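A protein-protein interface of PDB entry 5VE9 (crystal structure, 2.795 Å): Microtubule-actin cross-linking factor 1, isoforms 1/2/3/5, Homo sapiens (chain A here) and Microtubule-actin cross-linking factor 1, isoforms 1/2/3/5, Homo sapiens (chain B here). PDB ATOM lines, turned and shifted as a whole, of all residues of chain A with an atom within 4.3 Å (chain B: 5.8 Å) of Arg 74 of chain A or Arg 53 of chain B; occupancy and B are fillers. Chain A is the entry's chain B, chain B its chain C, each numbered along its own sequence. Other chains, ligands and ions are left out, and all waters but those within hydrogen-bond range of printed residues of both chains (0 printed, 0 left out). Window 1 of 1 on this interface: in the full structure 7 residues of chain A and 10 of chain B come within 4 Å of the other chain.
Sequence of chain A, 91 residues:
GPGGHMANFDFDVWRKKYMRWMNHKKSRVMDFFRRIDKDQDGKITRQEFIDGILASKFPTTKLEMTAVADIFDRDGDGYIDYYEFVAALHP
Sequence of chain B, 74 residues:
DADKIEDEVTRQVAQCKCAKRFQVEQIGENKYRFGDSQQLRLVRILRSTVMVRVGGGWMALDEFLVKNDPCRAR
The guanidinium group (NH2) of Arg 53 of chain B is in hydrogen-bond range of the backbone carbonyl oxygen (O) of Ile 71 of chain A, at 2.5 Å.
The backbone NH (N) of Gly 55 of chain B lies close to the guanidinium group (NH2) of Arg 74 of chain A (3.1 Å).
N of Arg 74 of chain A lies close to OE2 of Glu 84 of chain A (3.1 Å).
NH1 of Arg 41 of chain B is in hydrogen-bond range of O of Arg 53 of chain B (2.6 Å).
O of Leu 42 of chain B lies within hydrogen-bond range of N of Arg 53 of chain B (3.0 Å).
Asp 70 of chain A touches Arg 53 of chain B.
Arg 53 of chain B touches Asp 73 of chain A.
Arg 41 of chain B touches Arg 74 of chain A (NH2 to NH2, 3.9 Å).
Arg 74 of chain A touches Leu 42 of chain B.
Arg 74 of chain A touches Arg 53 of chain B (O to CG, 3.4 Å).
Arg 74 of chain A touches Val 54 of chain B (NH2 to C, 3.4 Å).
Asp 75 of chain A touches Leu 42 of chain B (C to CD1, 3.9 Å).
Printed residues of chain B within 4 Å of Asp 70 of chain A: Arg 53 (3.8 Å).
Of the printed residues of chain B, Ile 71 of chain A touches Arg 53.
Of the printed residues of chain B, Asp 73 of chain A touches Arg 53.
Of the printed residues of chain A, Leu 42 of chain B touches Arg 74 and Asp 75.
Val 43 of chain B touches none of the printed residues of chain A.
Of the printed residues of chain A, Arg 53 of chain B touches Asp 70, Ile 71, Asp 73 and Arg 74.
Phe 64 of chain B touches none of the printed residues of chain A.
The nearest residue of chain B that does not touch Arg 74 of chain A is Gln 39 of chain B (4.9 Å).
The nearest printed residue of chain A that does not touch Arg 53 of chain B is Phe 72 of chain A (4.7 Å).
Hydrophobic or aromatic side chains of chain B that line the printed part of chain A: Leu 42.
Of the 7 printed residues of chain A, 5 touch a printed residue of chain B.
Along chain A the printed residues that touch a printed residue of chain B span positions 70 to 75.
Among the printed residues, no Asp or Glu carboxylate lies within 4 Å of a Lys or Arg side-chain nitrogen of the other chain.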
ATOM      1  N   ASP A  70      16.337   2.835  -4.063  1.00  0.00           N
ATOM      2  CA  ASP A  70      17.120   2.273  -2.967  1.00  0.00           C
ATOM      3  C   ASP A  70      18.089   1.224  -3.500  1.00  0.00           C
ATOM      4  O   ASP A  70      19.244   1.153  -3.073  1.00  0.00           O
ATOM      5  CB  ASP A  70      16.219   1.643  -1.903  1.00  0.00           C
ATOM      6  CG  ASP A  70      16.998   1.177  -0.685  1.00  0.00           C
ATOM      7  OD1 ASP A  70      17.864   1.935  -0.202  1.00  0.00           O
ATOM      8  OD2 ASP A  70      16.751   0.046  -0.214  1.00  0.00           O
ATOM      9  N   ILE A  71      17.610   0.410  -4.436  1.00  0.00           N
ATOM     10  CA  ILE A  71      18.421  -0.654  -5.017  1.00  0.00           C
ATOM     11  C   ILE A  71      19.518  -0.105  -5.932  1.00  0.00           C
ATOM     12  O   ILE A  71      20.670  -0.523  -5.843  1.00  0.00           O
ATOM     13  CB  ILE A  71      17.552  -1.650  -5.810  1.00  0.00           C
ATOM     14  CG1 ILE A  71      16.641  -2.412  -4.847  1.00  0.00           C
ATOM     15  CG2 ILE A  71      18.438  -2.614  -6.599  1.00  0.00           C
ATOM     16  CD1 ILE A  71      15.658  -3.339  -5.509  1.00  0.00           C
ATOM     17  N   PHE A  72      19.152   0.817  -6.819  1.00  0.00           N
ATOM     18  CA  PHE A  72      20.123   1.457  -7.702  1.00  0.00           C
ATOM     19  C   PHE A  72      21.282   2.038  -6.906  1.00  0.00           C
ATOM     20  O   PHE A  72      22.439   1.936  -7.304  1.00  0.00           O
ATOM     21  CB  PHE A  72      19.464   2.565  -8.526  1.00  0.00           C
ATOM     22  CG  PHE A  72      18.894   2.092  -9.830  1.00  0.00           C
ATOM     23  CD1 PHE A  72      19.642   2.172 -10.995  1.00  0.00           C
ATOM     24  CD2 PHE A  72      17.616   1.565  -9.893  1.00  0.00           C
ATOM     25  CE1 PHE A  72      19.121   1.736 -12.198  1.00  0.00           C
ATOM     26  CE2 PHE A  72      17.092   1.126 -11.091  1.00  0.00           C
ATOM     27  CZ  PHE A  72      17.847   1.212 -12.247  1.00  0.00           C
ATOM     28  N   ASP A  73      20.954   2.644  -5.773  1.00  0.00           N
ATOM     29  CA  ASP A  73      21.955   3.254  -4.915  1.00  0.00           C
ATOM     30  C   ASP A  73      22.593   2.191  -4.014  1.00  0.00           C
ATOM     31  O   ASP A  73      22.153   1.983  -2.883  1.00  0.00           O
ATOM     32  CB  ASP A  73      21.316   4.371  -4.086  1.00  0.00           C
ATOM     33  CG  ASP A  73      22.328   5.161  -3.295  1.00  0.00           C
ATOM     34  OD1 ASP A  73      23.532   5.051  -3.606  1.00  0.00           O
ATOM     35  OD2 ASP A  73      21.926   5.891  -2.364  1.00  0.00           O
ATOM     36  N   ARG A  74      23.623   1.515  -4.524  1.00  0.00           N
ATOM     37  CA  ARG A  74      24.214   0.368  -3.826  1.00  0.00           C
ATOM     38  C   ARG A  74      24.860   0.753  -2.495  1.00  0.00           C
ATOM     39  O   ARG A  74      24.743   0.020  -1.513  1.00  0.00           O
ATOM     40  CB  ARG A  74      25.249  -0.336  -4.710  1.00  0.00           C
ATOM     41  CG  ARG A  74      26.023  -1.418  -3.963  1.00  0.00           C
ATOM     42  CD  ARG A  74      26.841  -2.313  -4.880  1.00  0.00           C
ATOM     43  NE  ARG A  74      27.543  -3.339  -4.112  1.00  0.00           N
ATOM     44  CZ  ARG A  74      28.190  -4.371  -4.645  1.00  0.00           C
ATOM     45  NH1 ARG A  74      28.233  -4.529  -5.960  1.00  0.00           N
ATOM     46  NH2 ARG A  74      28.794  -5.247  -3.855  1.00  0.00           N
ATOM     47  N   ASP A  75      25.557   1.885  -2.465  1.00  0.00           N
ATOM     48  CA  ASP A  75      26.011   2.461  -1.204  1.00  0.00           C
ATOM     49  C   ASP A  75      24.889   3.370  -0.691  1.00  0.00           C
ATOM     50  O   ASP A  75      23.865   3.519  -1.357  1.00  0.00           O
ATOM     51  CB  ASP A  75      27.332   3.225  -1.374  1.00  0.00           C
ATOM     52  CG  ASP A  75      27.352   4.105  -2.609  1.00  0.00           C
ATOM     53  OD1 ASP A  75      26.265   4.466  -3.101  1.00  0.00           O
ATOM     54  OD2 ASP A  75      28.458   4.439  -3.085  1.00  0.00           O
ATOM     55  N   GLU A  84      26.557   2.723 -11.020  1.00  0.00           N
ATOM     56  CA  GLU A  84      25.444   2.090 -10.325  1.00  0.00           C
ATOM     57  C   GLU A  84      24.272   1.901 -11.277  1.00  0.00           C
ATOM     58  O   GLU A  84      23.586   0.880 -11.247  1.00  0.00           O
ATOM     59  CB  GLU A  84      25.019   2.932  -9.126  1.00  0.00           C
ATOM     60  CG  GLU A  84      25.917   2.764  -7.918  1.00  0.00           C
ATOM     61  CD  GLU A  84      25.629   3.775  -6.818  1.00  0.00           C
ATOM     62  OE1 GLU A  84      25.273   4.928  -7.138  1.00  0.00           O
ATOM     63  OE2 GLU A  84      25.761   3.416  -5.632  1.00  0.00           O
ATOM     64  N   GLN B  39      36.175  -0.946   1.667  1.00  0.00           N
ATOM     65  CA  GLN B  39      35.196  -0.017   1.141  1.00  0.00           C
ATOM     66  C   GLN B  39      33.961   0.047   2.035  1.00  0.00           C
ATOM     67  O   GLN B  39      33.801  -0.753   2.959  1.00  0.00           O
ATOM     68  CB  GLN B  39      34.795  -0.449  -0.269  1.00  0.00           C
ATOM     69  CG  GLN B  39      33.683  -1.500  -0.294  1.00  0.00           C
ATOM     70  CD  GLN B  39      33.646  -2.300  -1.583  1.00  0.00           C
ATOM     71  OE1 GLN B  39      34.686  -2.693  -2.115  1.00  0.00           O
ATOM     72  NE2 GLN B  39      32.443  -2.549  -2.091  1.00  0.00           N
ATOM     73  N   ARG B  41      30.127  -0.398   2.996  1.00  0.00           N
ATOM     74  CA  ARG B  41      29.055  -1.346   2.689  1.00  0.00           C
ATOM     75  C   ARG B  41      27.824  -1.140   3.567  1.00  0.00           C
ATOM     76  O   ARG B  41      27.941  -0.831   4.753  1.00  0.00           O
ATOM     77  CB  ARG B  41      29.560  -2.781   2.854  1.00  0.00           C
ATOM     78  CG  ARG B  41      30.421  -3.267   1.707  1.00  0.00           C
ATOM     79  CD  ARG B  41      30.968  -4.653   1.985  1.00  0.00           C
ATOM     80  NE  ARG B  41      31.524  -5.274   0.786  1.00  0.00           N
ATOM     81  CZ  ARG B  41      30.801  -5.899  -0.138  1.00  0.00           C
ATOM     82  NH1 ARG B  41      29.482  -5.987  -0.013  1.00  0.00           N
ATOM     83  NH2 ARG B  41      31.398  -6.434  -1.194  1.00  0.00           N
ATOM     84  N   LEU B  42      26.646  -1.328   2.979  1.00  0.00           N
ATOM     85  CA  LEU B  42      25.399  -1.183   3.720  1.00  0.00           C
ATOM     86  C   LEU B  42      25.133  -2.420   4.566  1.00  0.00           C
ATOM     87  O   LEU B  42      25.486  -3.538   4.181  1.00  0.00           O
ATOM     88  CB  LEU B  42      24.221  -0.940   2.775  1.00  0.00           C
ATOM     89  CG  LEU B  42      24.193   0.398   2.035  1.00  0.00           C
ATOM     90  CD1 LEU B  42      23.004   0.445   1.092  1.00  0.00           C
ATOM     91  CD2 LEU B  42      24.150   1.561   3.016  1.00  0.00           C
ATOM     92  N   VAL B  43      24.509  -2.205   5.719  1.00  0.00           N
ATOM     93  CA  VAL B  43      24.148  -3.291   6.621  1.00  0.00           C
ATOM     94  C   VAL B  43      22.779  -3.015   7.223  1.00  0.00           C
ATOM     95  O   VAL B  43      22.598  -2.040   7.953  1.00  0.00           O
ATOM     96  CB  VAL B  43      25.177  -3.463   7.752  1.00  0.00           C
ATOM     97  CG1 VAL B  43      24.789  -4.624   8.659  1.00  0.00           C
ATOM     98  CG2 VAL B  43      26.565  -3.681   7.175  1.00  0.00           C
ATOM     99  N   MET B  51      21.750  -8.402   7.109  1.00  0.00           N
ATOM    100  CA  MET B  51      21.978  -8.462   5.672  1.00  0.00           C
ATOM    101  C   MET B  51      22.983  -7.402   5.248  1.00  0.00           C
ATOM    102  O   MET B  51      22.843  -6.231   5.601  1.00  0.00           O
ATOM    103  CB  MET B  51      20.665  -8.270   4.915  1.00  0.00           C
ATOM    104  CG  MET B  51      19.553  -9.208   5.357  1.00  0.00           C
ATOM    105  SD  MET B  51      19.893 -10.945   5.006  1.00  0.00           S
ATOM    106  CE  MET B  51      19.708 -10.983   3.225  1.00  0.00           C
ATOM    107  N   VAL B  52      23.993  -7.826   4.491  1.00  0.00           N
ATOM    108  CA  VAL B  52      25.013  -6.921   3.975  1.00  0.00           C
ATOM    109  C   VAL B  52      24.806  -6.739   2.475  1.00  0.00           C
ATOM    110  O   VAL B  52      24.414  -7.678   1.780  1.00  0.00           O
ATOM    111  CB  VAL B  52      26.430  -7.452   4.250  1.00  0.00           C
ATOM    112  CG1 VAL B  52      27.465  -6.376   3.961  1.00  0.00           C
ATOM    113  CG2 VAL B  52      26.542  -7.922   5.691  1.00  0.00           C
ATOM    114  N   ARG B  53      25.066  -5.537   1.975  1.00  0.00           N
ATOM    115  CA  ARG B  53      24.795  -5.227   0.576  1.00  0.00           C
ATOM    116  C   ARG B  53      25.910  -5.711  -0.347  1.00  0.00           C
ATOM    117  O   ARG B  53      27.037  -5.214  -0.288  1.00  0.00           O
ATOM    118  CB  ARG B  53      24.587  -3.720   0.400  1.00  0.00           C
ATOM    119  CG  ARG B  53      24.293  -3.277  -1.032  1.00  0.00           C
ATOM    120  CD  ARG B  53      23.073  -3.977  -1.597  1.00  0.00           C
ATOM    121  NE  ARG B  53      22.817  -3.619  -2.989  1.00  0.00           N
ATOM    122  CZ  ARG B  53      22.114  -2.560  -3.377  1.00  0.00           C
ATOM    123  NH1 ARG B  53      21.595  -1.727  -2.481  1.00  0.00           N
ATOM    124  NH2 ARG B  53      21.936  -2.326  -4.670  1.00  0.00           N
ATOM    125  N   VAL B  54      25.582  -6.680  -1.199  1.00  0.00           N
ATOM    126  CA  VAL B  54      26.528  -7.226  -2.168  1.00  0.00           C
ATOM    127  C   VAL B  54      25.962  -7.084  -3.586  1.00  0.00           C
ATOM    128  O   VAL B  54      24.819  -6.664  -3.761  1.00  0.00           O
ATOM    129  CB  VAL B  54      26.857  -8.705  -1.863  1.00  0.00           C
ATOM    130  CG1 VAL B  54      27.551  -8.819  -0.509  1.00  0.00           C
ATOM    131  CG2 VAL B  54      25.599  -9.566  -1.894  1.00  0.00           C
ATOM    132  N   GLY B  55      26.769  -7.421  -4.588  1.00  0.00           N
ATOM    133  CA  GLY B  55      26.412  -7.213  -5.984  1.00  0.00           C
ATOM    134  C   GLY B  55      25.027  -7.680  -6.397  1.00  0.00           C
ATOM    135  O   GLY B  55      24.199  -6.874  -6.827  1.00  0.00           O
ATOM    136  N   GLY B  56      24.769  -8.978  -6.267  1.00  0.00           N
ATOM    137  CA  GLY B  56      23.508  -9.553  -6.706  1.00  0.00           C
ATOM    138  C   GLY B  56      22.328  -9.278  -5.792  1.00  0.00           C
ATOM    139  O   GLY B  56      21.228  -9.782  -6.030  1.00  0.00           O
ATOM    140  N   GLY B  57      22.547  -8.482  -4.750  1.00  0.00           N
ATOM    141  CA  GLY B  57      21.492  -8.147  -3.810  1.00  0.00           C
ATOM    142  C   GLY B  57      22.008  -8.057  -2.389  1.00  0.00           C
ATOM    143  O   GLY B  57      22.839  -7.208  -2.079  1.00  0.00           O
ATOM    144  N   TRP B  58      21.513  -8.935  -1.522  1.00  0.00           N
ATOM    145  CA  TRP B  58      21.915  -8.933  -0.121  1.00  0.00           C
ATOM    146  C   TRP B  58      22.368 -10.317   0.320  1.00  0.00           C
ATOM    147  O   TRP B  58      21.866 -11.334  -0.160  1.00  0.00           O
ATOM    148  CB  TRP B  58      20.764  -8.437   0.753  1.00  0.00           C
ATOM    149  CG  TRP B  58      20.444  -6.993   0.510  1.00  0.00           C
ATOM    150  CD1 TRP B  58      19.731  -6.475  -0.531  1.00  0.00           C
ATOM    151  CD2 TRP B  58      20.835  -5.878   1.323  1.00  0.00           C
ATOM    152  NE1 TRP B  58      19.653  -5.109  -0.418  1.00  0.00           N
ATOM    153  CE2 TRP B  58      20.324  -4.716   0.711  1.00  0.00           C
ATOM    154  CE3 TRP B  58      21.569  -5.748   2.506  1.00  0.00           C
ATOM    155  CZ2 TRP B  58      20.515  -3.444   1.245  1.00  0.00           C
ATOM    156  CZ3 TRP B  58      21.759  -4.483   3.036  1.00  0.00           C
ATOM    157  CH2 TRP B  58      21.236  -3.348   2.403  1.00  0.00           C
ATOM    158  N   MET B  59      23.330 -10.335   1.238  1.00  0.00           N
ATOM    159  CA  MET B  59      23.937 -11.570   1.713  1.00  0.00           C
ATOM    160  C   MET B  59      23.859 -11.639   3.234  1.00  0.00           C
ATOM    161  O   MET B  59      24.068 -10.635   3.918  1.00  0.00           O
ATOM    162  CB  MET B  59      25.392 -11.654   1.248  1.00  0.00           C
ATOM    163  CG  MET B  59      26.016 -13.029   1.386  1.00  0.00           C
ATOM    164  SD  MET B  59      27.783 -13.039   1.026  1.00  0.00           S
ATOM    165  CE  MET B  59      27.795 -12.739  -0.739  1.00  0.00           C
ATOM    166  N   PHE B  64      28.647 -13.634   4.335  1.00  0.00           N
ATOM    167  CA  PHE B  64      29.546 -12.533   4.003  1.00  0.00           C
ATOM    168  C   PHE B  64      30.914 -12.725   4.654  1.00  0.00           C
ATOM    169  O   PHE B  64      31.948 -12.610   3.993  1.00  0.00           O
ATOM    170  CB  PHE B  64      28.946 -11.193   4.439  1.00  0.00           C
ATOM    171  CG  PHE B  64      29.857 -10.017   4.207  1.00  0.00           C
ATOM    172  CD1 PHE B  64      29.954  -9.435   2.953  1.00  0.00           C
ATOM    173  CD2 PHE B  64      30.617  -9.494   5.242  1.00  0.00           C
ATOM    174  CE1 PHE B  64      30.792  -8.355   2.735  1.00  0.00           C
ATOM    175  CE2 PHE B  64      31.457  -8.413   5.030  1.00  0.00           C
ATOM    176  CZ  PHE B  64      31.542  -7.842   3.775  1.00  0.00           C
